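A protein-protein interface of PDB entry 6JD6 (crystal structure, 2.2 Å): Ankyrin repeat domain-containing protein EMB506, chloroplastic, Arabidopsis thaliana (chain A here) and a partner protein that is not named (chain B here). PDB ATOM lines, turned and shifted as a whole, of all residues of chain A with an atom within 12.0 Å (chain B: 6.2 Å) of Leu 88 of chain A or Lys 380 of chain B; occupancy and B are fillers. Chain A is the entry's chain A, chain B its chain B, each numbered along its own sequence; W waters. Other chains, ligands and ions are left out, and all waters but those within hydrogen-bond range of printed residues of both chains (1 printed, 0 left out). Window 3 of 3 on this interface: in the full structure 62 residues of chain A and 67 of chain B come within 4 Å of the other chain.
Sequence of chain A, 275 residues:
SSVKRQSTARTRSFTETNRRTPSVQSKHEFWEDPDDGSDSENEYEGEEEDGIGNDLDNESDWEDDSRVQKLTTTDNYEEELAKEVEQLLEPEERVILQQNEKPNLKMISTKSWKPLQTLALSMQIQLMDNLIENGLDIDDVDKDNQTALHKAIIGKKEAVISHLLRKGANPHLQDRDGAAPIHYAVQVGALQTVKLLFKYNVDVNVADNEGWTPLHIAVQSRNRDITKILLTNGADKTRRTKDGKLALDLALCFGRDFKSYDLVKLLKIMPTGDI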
ATOM      1  N   TYR A  77     -39.705  -3.064 -17.563  1.00  0.00           N
ATOM      2  CA  TYR A  77     -38.262  -2.895 -17.644  1.00  0.00           C
ATOM      3  C   TYR A  77     -37.818  -2.869 -19.099  1.00  0.00           C
ATOM      4  O   TYR A  77     -36.920  -2.113 -19.460  1.00  0.00           O
ATOM      5  CB  TYR A  77     -37.514  -4.000 -16.892  1.00  0.00           C
ATOM      6  CG  TYR A  77     -36.012  -3.826 -16.964  1.00  0.00           C
ATOM      7  CD1 TYR A  77     -35.360  -2.923 -16.134  1.00  0.00           C
ATOM      8  CD2 TYR A  77     -35.250  -4.543 -17.877  1.00  0.00           C
ATOM      9  CE1 TYR A  77     -33.990  -2.743 -16.203  1.00  0.00           C
ATOM     10  CE2 TYR A  77     -33.880  -4.373 -17.953  1.00  0.00           C
ATOM     11  CZ  TYR A  77     -33.255  -3.471 -17.114  1.00  0.00           C
ATOM     12  OH  TYR A  77     -31.890  -3.294 -17.182  1.00  0.00           O
ATOM     13  N   GLU A  79     -39.695  -1.941 -21.749  1.00  0.00           N
ATOM     14  CA  GLU A  79     -40.161  -0.685 -22.321  1.00  0.00           C
ATOM     15  C   GLU A  79     -39.342   0.492 -21.809  1.00  0.00           C
ATOM     16  O   GLU A  79     -39.056   1.426 -22.554  1.00  0.00           O
ATOM     17  CB  GLU A  79     -41.648  -0.467 -22.027  1.00  0.00           C
ATOM     18  CG  GLU A  79     -42.566  -1.378 -22.821  1.00  0.00           C
ATOM     19  CD  GLU A  79     -42.268  -1.341 -24.308  1.00  0.00           C
ATOM     20  OE1 GLU A  79     -42.698  -0.378 -24.978  1.00  0.00           O
ATOM     21  OE2 GLU A  79     -41.597  -2.270 -24.806  1.00  0.00           O
ATOM     22  N   GLU A  80     -38.972   0.443 -20.534  1.00  0.00           N
ATOM     23  CA  GLU A  80     -38.169   1.499 -19.938  1.00  0.00           C
ATOM     24  C   GLU A  80     -36.782   1.514 -20.562  1.00  0.00           C
ATOM     25  O   GLU A  80     -36.252   2.574 -20.886  1.00  0.00           O
ATOM     26  CB  GLU A  80     -38.056   1.309 -18.424  1.00  0.00           C
ATOM     27  CG  GLU A  80     -37.271   2.403 -17.720  1.00  0.00           C
ATOM     28  CD  GLU A  80     -37.123   2.149 -16.233  1.00  0.00           C
ATOM     29  OE1 GLU A  80     -37.100   0.968 -15.830  1.00  0.00           O
ATOM     30  OE2 GLU A  80     -37.037   3.133 -15.468  1.00  0.00           O
ATOM     31  N   LEU A  81     -36.206   0.327 -20.732  1.00  0.00           N
ATOM     32  CA  LEU A  81     -34.882   0.183 -21.312  1.00  0.00           C
ATOM     33  C   LEU A  81     -34.902   0.546 -22.791  1.00  0.00           C
ATOM     34  O   LEU A  81     -33.995   1.218 -23.281  1.00  0.00           O
ATOM     35  CB  LEU A  81     -34.375  -1.247 -21.121  1.00  0.00           C
ATOM     36  CG  LEU A  81     -32.996  -1.613 -21.672  1.00  0.00           C
ATOM     37  CD1 LEU A  81     -31.917  -0.776 -21.010  1.00  0.00           C
ATOM     38  CD2 LEU A  81     -32.719  -3.104 -21.480  1.00  0.00           C
ATOM     39  N   ALA A  82     -35.938   0.097 -23.497  1.00  0.00           N
ATOM     40  CA  ALA A  82     -36.102   0.422 -24.913  1.00  0.00           C
ATOM     41  C   ALA A  82     -36.108   1.935 -25.134  1.00  0.00           C
ATOM     42  O   ALA A  82     -35.449   2.440 -26.048  1.00  0.00           O
ATOM     43  CB  ALA A  82     -37.383  -0.199 -25.459  1.00  0.00           C
ATOM     44  N   LYS A  83     -36.844   2.648 -24.287  1.00  0.00           N
ATOM     45  CA  LYS A  83     -36.902   4.105 -24.355  1.00  0.00           C
ATOM     46  C   LYS A  83     -35.550   4.745 -24.039  1.00  0.00           C
ATOM     47  O   LYS A  83     -35.126   5.669 -24.732  1.00  0.00           O
ATOM     48  CB  LYS A  83     -37.974   4.658 -23.410  1.00  0.00           C
ATOM     49  CG  LYS A  83     -38.039   6.182 -23.405  1.00  0.00           C
ATOM     50  CD  LYS A  83     -38.985   6.730 -22.337  1.00  0.00           C
ATOM     51  CE  LYS A  83     -38.953   8.256 -22.325  1.00  0.00           C
ATOM     52  NZ  LYS A  83     -39.755   8.856 -21.223  1.00  0.00           N
ATOM     53  N   GLU A  84     -34.888   4.259 -22.990  1.00  0.00           N
ATOM     54  CA  GLU A  84     -33.564   4.757 -22.609  1.00  0.00           C
ATOM     55  C   GLU A  84     -32.590   4.705 -23.776  1.00  0.00           C
ATOM     56  O   GLU A  84     -31.856   5.657 -24.034  1.00  0.00           O
ATOM     57  CB  GLU A  84     -32.986   3.948 -21.450  1.00  0.00           C
ATOM     58  CG  GLU A  84     -33.607   4.247 -20.096  1.00  0.00           C
ATOM     59  CD  GLU A  84     -32.988   3.421 -18.985  1.00  0.00           C
ATOM     60  OE1 GLU A  84     -31.962   2.753 -19.242  1.00  0.00           O
ATOM     61  OE2 GLU A  84     -33.527   3.440 -17.856  1.00  0.00           O
ATOM     62  N   VAL A  85     -32.596   3.582 -24.483  1.00  0.00           N
ATOM     63  CA  VAL A  85     -31.685   3.378 -25.597  1.00  0.00           C
ATOM     64  C   VAL A  85     -32.043   4.247 -26.804  1.00  0.00           C
ATOM     65  O   VAL A  85     -31.163   4.843 -27.427  1.00  0.00           O
ATOM     66  CB  VAL A  85     -31.642   1.898 -25.999  1.00  0.00           C
ATOM     67  CG1 VAL A  85     -30.824   1.714 -27.253  1.00  0.00           C
ATOM     68  CG2 VAL A  85     -31.070   1.068 -24.857  1.00  0.00           C
ATOM     69  N   GLU A  86     -33.331   4.327 -27.124  1.00  0.00           N
ATOM     70  CA  GLU A  86     -33.786   5.147 -28.242  1.00  0.00           C
ATOM     71  C   GLU A  86     -33.416   6.611 -28.051  1.00  0.00           C
ATOM     72  O   GLU A  86     -33.136   7.320 -29.020  1.00  0.00           O
ATOM     73  CB  GLU A  86     -35.295   5.002 -28.438  1.00  0.00           C
ATOM     74  CG  GLU A  86     -35.707   3.639 -28.976  1.00  0.00           C
ATOM     75  CD  GLU A  86     -37.197   3.392 -28.866  1.00  0.00           C
ATOM     76  OE1 GLU A  86     -37.930   4.329 -28.485  1.00  0.00           O
ATOM     77  OE2 GLU A  86     -37.631   2.258 -29.155  1.00  0.00           O
ATOM     78  N   GLN A  87     -33.410   7.052 -26.796  1.00  0.00           N
ATOM     79  CA  GLN A  87     -33.050   8.426 -26.449  1.00  0.00           C
ATOM     80  C   GLN A  87     -31.584   8.736 -26.744  1.00  0.00           C
ATOM     81  O   GLN A  87     -31.205   9.897 -26.873  1.00  0.00           O
ATOM     82  CB  GLN A  87     -33.342   8.685 -24.973  1.00  0.00           C
ATOM     83  CG  GLN A  87     -34.812   8.899 -24.658  1.00  0.00           C
ATOM     84  CD  GLN A  87     -35.073   9.015 -23.167  1.00  0.00           C
ATOM     85  OE1 GLN A  87     -34.496   8.276 -22.365  1.00  0.00           O
ATOM     86  NE2 GLN A  87     -35.940   9.945 -22.790  1.00  0.00           N
ATOM     87  N   LEU A  88     -30.772   7.688 -26.846  1.00  0.00           N
ATOM     88  CA  LEU A  88     -29.344   7.820 -27.110  1.00  0.00           C
ATOM     89  C   LEU A  88     -29.013   7.803 -28.601  1.00  0.00           C
ATOM     90  O   LEU A  88     -27.916   8.191 -29.000  1.00  0.00           O
ATOM     91  CB  LEU A  88     -28.573   6.683 -26.429  1.00  0.00           C
ATOM     92  CG  LEU A  88     -28.582   6.626 -24.904  1.00  0.00           C
ATOM     93  CD1 LEU A  88     -28.056   5.287 -24.415  1.00  0.00           C
ATOM     94  CD2 LEU A  88     -27.757   7.768 -24.334  1.00  0.00           C
ATOM     95  N   LEU A  89     -29.957   7.353 -29.420  1.00  0.00           N
ATOM     96  CA  LEU A  89     -29.674   7.095 -30.831  1.00  0.00           C
ATOM     97  C   LEU A  89     -29.805   8.322 -31.729  1.00  0.00           C
ATOM     98  O   LEU A  89     -30.584   9.232 -31.457  1.00  0.00           O
ATOM     99  CB  LEU A  89     -30.576   5.978 -31.364  1.00  0.00           C
ATOM    100  CG  LEU A  89     -30.481   4.610 -30.686  1.00  0.00           C
ATOM    101  CD1 LEU A  89     -31.427   3.621 -31.349  1.00  0.00           C
ATOM    102  CD2 LEU A  89     -29.058   4.083 -30.723  1.00  0.00           C
ATOM    103  N   GLU A  90     -29.029   8.328 -32.809  1.00  0.00           N
ATOM    104  CA  GLU A  90     -29.205   9.296 -33.883  1.00  0.00           C
ATOM    105  C   GLU A  90     -30.512   8.962 -34.596  1.00  0.00           C
ATOM    106  O   GLU A  90     -30.981   7.825 -34.515  1.00  0.00           O
ATOM    107  CB  GLU A  90     -28.034   9.192 -34.863  1.00  0.00           C
ATOM    108  CG  GLU A  90     -26.667   9.381 -34.224  1.00  0.00           C
ATOM    109  CD  GLU A  90     -26.403  10.821 -33.847  1.00  0.00           C
ATOM    110  OE1 GLU A  90     -26.477  11.690 -34.742  1.00  0.00           O
ATOM    111  OE2 GLU A  90     -26.130  11.089 -32.656  1.00  0.00           O
ATOM    112  N   PRO A  91     -31.111   9.943 -35.291  1.00  0.00           N
ATOM    113  CA  PRO A  91     -32.349   9.674 -36.038  1.00  0.00           C
ATOM    114  C   PRO A  91     -32.196   8.524 -37.042  1.00  0.00           C
ATOM    115  O   PRO A  91     -33.104   7.707 -37.184  1.00  0.00           O
ATOM    116  CB  PRO A  91     -32.602  10.991 -36.774  1.00  0.00           C
ATOM    117  CG  PRO A  91     -31.961  12.027 -35.910  1.00  0.00           C
ATOM    118  CD  PRO A  91     -30.731  11.366 -35.350  1.00  0.00           C
ATOM    119  N   GLU A  92     -31.049   8.456 -37.707  1.00  0.00           N
ATOM    120  CA  GLU A  92     -30.798   7.434 -38.718  1.00  0.00           C
ATOM    121  C   GLU A  92     -30.730   6.042 -38.098  1.00  0.00           C
ATOM    122  O   GLU A  92     -31.203   5.065 -38.682  1.00  0.00           O
ATOM    123  CB  GLU A  92     -29.497   7.733 -39.473  1.00  0.00           C
ATOM    124  CG  GLU A  92     -29.492   9.060 -40.235  1.00  0.00           C
ATOM    125  CD  GLU A  92     -29.371  10.275 -39.326  1.00  0.00           C
ATOM    126  OE1 GLU A  92     -30.077  11.276 -39.577  1.00  0.00           O
ATOM    127  OE2 GLU A  92     -28.571  10.230 -38.366  1.00  0.00           O
ATOM    128  N   GLU A  93     -30.135   5.959 -36.913  1.00  0.00           N
ATOM    129  CA  GLU A  93     -30.038   4.697 -36.194  1.00  0.00           C
ATOM    130  C   GLU A  93     -31.417   4.258 -35.714  1.00  0.00           C
ATOM    131  O   GLU A  93     -31.752   3.075 -35.751  1.00  0.00           O
ATOM    132  CB  GLU A  93     -29.073   4.838 -35.017  1.00  0.00           C
ATOM    133  CG  GLU A  93     -27.642   5.136 -35.439  1.00  0.00           C
ATOM    134  CD  GLU A  93     -26.780   5.613 -34.288  1.00  0.00           C
ATOM    135  OE1 GLU A  93     -27.337   6.117 -33.291  1.00  0.00           O
ATOM    136  OE2 GLU A  93     -25.544   5.489 -34.379  1.00  0.00           O
ATOM    137  N   ARG A  94     -32.213   5.226 -35.275  1.00  0.00           N
ATOM    138  CA  ARG A  94     -33.578   4.984 -34.820  1.00  0.00           C
ATOM    139  C   ARG A  94     -34.443   4.381 -35.924  1.00  0.00           C
ATOM    140  O   ARG A  94     -35.219   3.455 -35.681  1.00  0.00           O
ATOM    141  CB  ARG A  94     -34.203   6.292 -34.336  1.00  0.00           C
ATOM    142  CG  ARG A  94     -34.631   6.297 -32.880  1.00  0.00           C
ATOM    143  CD  ARG A  94     -35.947   5.566 -32.683  1.00  0.00           C
ATOM    144  NE  ARG A  94     -36.793   6.228 -31.691  1.00  0.00           N
ATOM    145  CZ  ARG A  94     -38.051   5.886 -31.432  1.00  0.00           C
ATOM    146  NH1 ARG A  94     -38.616   4.883 -32.094  1.00  0.00           N
ATOM    147  NH2 ARG A  94     -38.747   6.548 -30.515  1.00  0.00           N
ATOM    148  N   VAL A  95     -34.315   4.914 -37.135  1.00  0.00           N
ATOM    149  CA  VAL A  95     -35.083   4.412 -38.270  1.00  0.00           C
ATOM    150  C   VAL A  95     -34.771   2.938 -38.548  1.00  0.00           C
ATOM    151  O   VAL A  95     -35.677   2.137 -38.771  1.00  0.00           O
ATOM    152  CB  VAL A  95     -34.849   5.261 -39.539  1.00  0.00           C
ATOM    153  CG1 VAL A  95     -35.435   4.571 -40.762  1.00  0.00           C
ATOM    154  CG2 VAL A  95     -35.450   6.653 -39.370  1.00  0.00           C
ATOM    155  N   ILE A  96     -33.494   2.577 -38.510  1.00  0.00           N
ATOM    156  CA  ILE A  96     -33.095   1.188 -38.725  1.00  0.00           C
ATOM    157  C   ILE A  96     -33.656   0.267 -37.640  1.00  0.00           C
ATOM    158  O   ILE A  96     -34.174  -0.814 -37.932  1.00  0.00           O
ATOM    159  CB  ILE A  96     -31.566   1.047 -38.774  1.00  0.00           C
ATOM    160  CG1 ILE A  96     -30.990   1.935 -39.881  1.00  0.00           C
ATOM    161  CG2 ILE A  96     -31.170  -0.412 -38.979  1.00  0.00           C
ATOM    162  CD1 ILE A  96     -29.486   1.820 -40.025  1.00  0.00           C
ATOM    163  N   LEU A  97     -33.555   0.706 -36.390  1.00  0.00           N
ATOM    164  CA  LEU A  97     -34.067  -0.063 -35.263  1.00  0.00           C
ATOM    165  C   LEU A  97     -35.565  -0.360 -35.399  1.00  0.00           C
ATOM    166  O   LEU A  97     -35.998  -1.497 -35.217  1.00  0.00           O
ATOM    167  CB  LEU A  97     -33.798   0.675 -33.949  1.00  0.00           C
ATOM    168  CG  LEU A  97     -34.263  -0.042 -32.680  1.00  0.00           C
ATOM    169  CD1 LEU A  97     -33.537  -1.369 -32.523  1.00  0.00           C
ATOM    170  CD2 LEU A  97     -34.059   0.839 -31.453  1.00  0.00           C
ATOM    171  N   LEU B 360     -22.236  -1.103 -33.088  1.00  0.00           N
ATOM    172  CA  LEU B 360     -23.535  -0.518 -32.773  1.00  0.00           C
ATOM    173  C   LEU B 360     -24.497  -0.647 -33.946  1.00  0.00           C
ATOM    174  O   LEU B 360     -25.660  -1.006 -33.763  1.00  0.00           O
ATOM    175  CB  LEU B 360     -23.416   0.949 -32.376  1.00  0.00           C
ATOM    176  CG  LEU B 360     -24.808   1.557 -32.147  1.00  0.00           C
ATOM    177  CD1 LEU B 360     -25.292   1.329 -30.718  1.00  0.00           C
ATOM    178  CD2 LEU B 360     -24.844   3.011 -32.524  1.00  0.00           C
ATOM    179  N   VAL B 375     -26.722  -4.186 -24.656  1.00  0.00           N
ATOM    180  CA  VAL B 375     -25.491  -4.020 -25.417  1.00  0.00           C
ATOM    181  C   VAL B 375     -25.450  -2.650 -26.083  1.00  0.00           C
ATOM    182  O   VAL B 375     -24.441  -1.949 -26.009  1.00  0.00           O
ATOM    183  CB  VAL B 375     -25.331  -5.124 -26.482  1.00  0.00           C
ATOM    184  CG1 VAL B 375     -24.184  -4.794 -27.422  1.00  0.00           C
ATOM    185  CG2 VAL B 375     -25.100  -6.460 -25.809  1.00  0.00           C
ATOM    186  N   MET B 376     -26.554  -2.270 -26.723  1.00  0.00           N
ATOM    187  CA  MET B 376     -26.663  -0.963 -27.371  1.00  0.00           C
ATOM    188  C   MET B 376     -26.346   0.162 -26.400  1.00  0.00           C
ATOM    189  O   MET B 376     -25.643   1.114 -26.742  1.00  0.00           O
ATOM    190  CB  MET B 376     -28.063  -0.759 -27.956  1.00  0.00           C
ATOM    191  CG  MET B 376     -28.427  -1.784 -29.012  1.00  0.00           C
ATOM    192  SD  MET B 376     -30.023  -1.522 -29.802  1.00  0.00           S
ATOM    193  CE  MET B 376     -29.870   0.197 -30.251  1.00  0.00           C
ATOM    194  N   LYS B 377     -26.867   0.038 -25.184  1.00  0.00           N
ATOM    195  CA  LYS B 377     -26.654   1.042 -24.148  1.00  0.00           C
ATOM    196  C   LYS B 377     -25.176   1.175 -23.799  1.00  0.00           C
ATOM    197  O   LYS B 377     -24.654   2.280 -23.690  1.00  0.00           O
ATOM    198  CB  LYS B 377     -27.473   0.690 -22.905  1.00  0.00           C
ATOM    199  CG  LYS B 377     -27.404   1.703 -21.781  1.00  0.00           C
ATOM    200  CD  LYS B 377     -28.662   1.629 -20.931  1.00  0.00           C
ATOM    201  CE  LYS B 377     -28.346   1.321 -19.480  1.00  0.00           C
ATOM    202  NZ  LYS B 377     -27.545   2.396 -18.842  1.00  0.00           N
ATOM    203  N   LEU B 378     -24.511   0.039 -23.625  1.00  0.00           N
ATOM    204  CA  LEU B 378     -23.075  -0.009 -23.379  1.00  0.00           C
ATOM    205  C   LEU B 378     -22.300   0.702 -24.485  1.00  0.00           C
ATOM    206  O   LEU B 378     -21.418   1.518 -24.218  1.00  0.00           O
ATOM    207  CB  LEU B 378     -22.623  -1.467 -23.314  1.00  0.00           C
ATOM    208  CG  LEU B 378     -21.942  -1.955 -22.039  1.00  0.00           C
ATOM    209  CD1 LEU B 378     -22.805  -1.657 -20.838  1.00  0.00           C
ATOM    210  CD2 LEU B 378     -21.670  -3.450 -22.147  1.00  0.00           C
ATOM    211  N   LEU B 379     -22.641   0.380 -25.730  1.00  0.00           N
ATOM    212  CA  LEU B 379     -21.971   0.949 -26.897  1.00  0.00           C
ATOM    213  C   LEU B 379     -22.136   2.469 -27.012  1.00  0.00           C
ATOM    214  O   LEU B 379     -21.185   3.172 -27.351  1.00  0.00           O
ATOM    215  CB  LEU B 379     -22.464   0.263 -28.169  1.00  0.00           C
ATOM    216  CG  LEU B 379     -22.061  -1.206 -28.309  1.00  0.00           C
ATOM    217  CD1 LEU B 379     -22.724  -1.838 -29.527  1.00  0.00           C
ATOM    218  CD2 LEU B 379     -20.546  -1.327 -28.402  1.00  0.00           C
ATOM    219  N   LYS B 380     -23.336   2.971 -26.725  1.00  0.00           N
ATOM    220  CA  LYS B 380     -23.601   4.408 -26.809  1.00  0.00           C
ATOM    221  C   LYS B 380     -23.033   5.177 -25.620  1.00  0.00           C
ATOM    222  O   LYS B 380     -22.595   6.317 -25.765  1.00  0.00           O
ATOM    223  CB  LYS B 380     -25.103   4.690 -26.919  1.00  0.00           C
ATOM    224  CG  LYS B 380     -25.770   4.103 -28.152  1.00  0.00           C
ATOM    225  CD  LYS B 380     -25.215   4.702 -29.431  1.00  0.00           C
ATOM    226  CE  LYS B 380     -25.440   6.193 -29.495  1.00  0.00           C
ATOM    227  NZ  LYS B 380     -25.216   6.729 -30.869  1.00  0.00           N
ATOM    228  N   GLU B 381     -23.048   4.557 -24.444  1.00  0.00           N
ATOM    229  CA  GLU B 381     -22.647   5.247 -23.221  1.00  0.00           C
ATOM    230  C   GLU B 381     -21.144   5.226 -22.943  1.00  0.00           C
ATOM    231  O   GLU B 381     -20.597   6.202 -22.433  1.00  0.00           O
ATOM    232  CB  GLU B 381     -23.421   4.709 -22.011  1.00  0.00           C
ATOM    233  CG  GLU B 381     -24.916   5.017 -22.056  1.00  0.00           C
ATOM    234  CD  GLU B 381     -25.623   4.736 -20.741  1.00  0.00           C
ATOM    235  OE1 GLU B 381     -25.013   4.095 -19.860  1.00  0.00           O
ATOM    236  OE2 GLU B 381     -26.789   5.165 -20.586  1.00  0.00           O
ATOM    237  N   PHE B 382     -20.480   4.121 -23.280  1.00  0.00           N
ATOM    238  CA  PHE B 382     -19.061   3.950 -22.943  1.00  0.00           C
ATOM    239  C   PHE B 382     -18.091   5.061 -23.385  1.00  0.00           C
ATOM    240  O   PHE B 382     -17.227   5.452 -22.602  1.00  0.00           O
ATOM    241  CB  PHE B 382     -18.525   2.578 -23.382  1.00  0.00           C
ATOM    242  CG  PHE B 382     -17.138   2.289 -22.877  1.00  0.00           C
ATOM    243  CD1 PHE B 382     -16.947   1.762 -21.607  1.00  0.00           C
ATOM    244  CD2 PHE B 382     -16.024   2.571 -23.659  1.00  0.00           C
ATOM    245  CE1 PHE B 382     -15.672   1.508 -21.129  1.00  0.00           C
ATOM    246  CE2 PHE B 382     -14.746   2.319 -23.190  1.00  0.00           C
ATOM    247  CZ  PHE B 382     -14.569   1.788 -21.922  1.00  0.00           C
ATOM    248  N   PRO B 383     -18.210   5.554 -24.635  1.00  0.00           N
ATOM    249  CA  PRO B 383     -17.297   6.626 -25.051  1.00  0.00           C
ATOM    250  C   PRO B 383     -17.415   7.864 -24.170  1.00  0.00           C
ATOM    251  O   PRO B 383     -16.427   8.568 -23.962  1.00  0.00           O
ATOM    252  CB  PRO B 383     -17.781   6.966 -26.463  1.00  0.00           C
ATOM    253  CG  PRO B 383     -18.424   5.739 -26.942  1.00  0.00           C
ATOM    254  CD  PRO B 383     -19.063   5.106 -25.751  1.00  0.00           C
ATOM    255  N   LEU B 384     -18.617   8.118 -23.664  1.00  0.00           N
ATOM    256  CA  LEU B 384     -18.873   9.284 -22.826  1.00  0.00           C
ATOM    257  C   LEU B 384     -18.214   9.149 -21.458  1.00  0.00           C
ATOM    258  O   LEU B 384     -17.911  10.146 -20.809  1.00  0.00           O
ATOM    259  CB  LEU B 384     -20.378   9.504 -22.663  1.00  0.00           C
ATOM    260  CG  LEU B 384     -21.151  10.246 -23.758  1.00  0.00           C
ATOM    261  CD1 LEU B 384     -20.388  10.321 -25.074  1.00  0.00           C
ATOM    262  CD2 LEU B 384     -22.517   9.605 -23.960  1.00  0.00           C
HETATM  263  O   HOH W   1     -25.514   9.225 -30.541  1.00  0.00           O
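The side-chain carboxylate of Glu 93 of chain A lies within salt-bridge range of the side-chain amino group of Lys 380 of chain B.
The side-chain carboxylate (OE1) of Glu 93 of chain A lies within hydrogen-bond range of the backbone NH (N) of Glu 90 of chain A (2.8 Å). The side-chain amino group (NZ) of Lys 377 of chain B is in salt-bridge range of the side-chain carboxylate (OE1) of Glu 381 of chain B, 3.2 Å away.
Among the printed residues, pairs that only touch across the chains: Glu 84 of chain A with Lys 377 of chain B (3.9 Å), Val 85 of chain A with Met 376 of chain B (3.5 Å), Leu 88 of chain A with Lys 380 of chain B (3.2 Å), Leu 88 of chain A with Glu 381 of chain B (3.9 Å), Leu 89 of chain A with Met 376 of chain B (3.9 Å) and Glu 93 of chain A with Leu 360 of chain B (3.2 Å).
Leu 81 of chain A touches none of the printed residues of chain B. Printed residues of chain B within 4 Å of Glu 84 of chain A: Lys 377. Of the printed residues of chain B, Val 85 of chain A touches Met 376 (3.5 Å). Leu 88 of chain A touches just these residues of chain B: Lys 380 (3.2 Å) and Glu 381 (3.9 Å). Printed residues of chain B within 4 Å of Leu 89 of chain A: Met 376 (3.9 Å). Of the printed residues of chain B, Glu 93 of chain A touches Leu 360 (3.2 Å) and Lys 380 (3.3 Å). Of chain A, only Glu 93 (3.2 Å) comes within 4 Å of Leu 360 of chain B. Of chain A, only Glu 84 comes within 4 Å of Lys 377 of chain B. No residue of chain A comes within 4 Å of Leu 379 of chain B. Of chain A, only Leu 88 and Glu 93 come within 4 Å of Lys 380 of chain B. Glu 381 of chain B touches one residue of chain A. No residue of chain A comes within 4 Å of Pro 383 of chain B. Leu 384 of chain B touches none of the printed residues of chain A. The nearest residue of chain B that does not touch Leu 88 of chain A is Lys 377 of chain B (4.5 Å). The nearest residue of chain A that does not touch Lys 380 of chain B is Leu 89 of chain A (4.1 Å). The nearest printed residue of chain B that does not touch Glu 93 of chain A is Met 376 of chain B (6.5 Å).
Of the 20 printed residues of chain A, 5 touch a printed residue of chain B. Hydrophobic or aromatic side chains of chain A that line the printed part of chain B: Val 85, Leu 88 and Leu 89. Among the printed residues, 7 pairs touch across the chains. Among the printed residues, Asp or Glu carboxylates within 4 Å of a Lys or Arg side-chain nitrogen of the other chain: Glu 93 of chain A with Lys 380 of chain B (3.3 Å).
Water W1 lies within hydrogen-bond range of the side-chain amino group of Lys 380 of chain B (2.5 Å), the side-chain carboxylate of Glu 90 of chain A (2.9 Å) and the backbone carbonyl oxygen of Leu 88 of chain A (3.0 Å).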
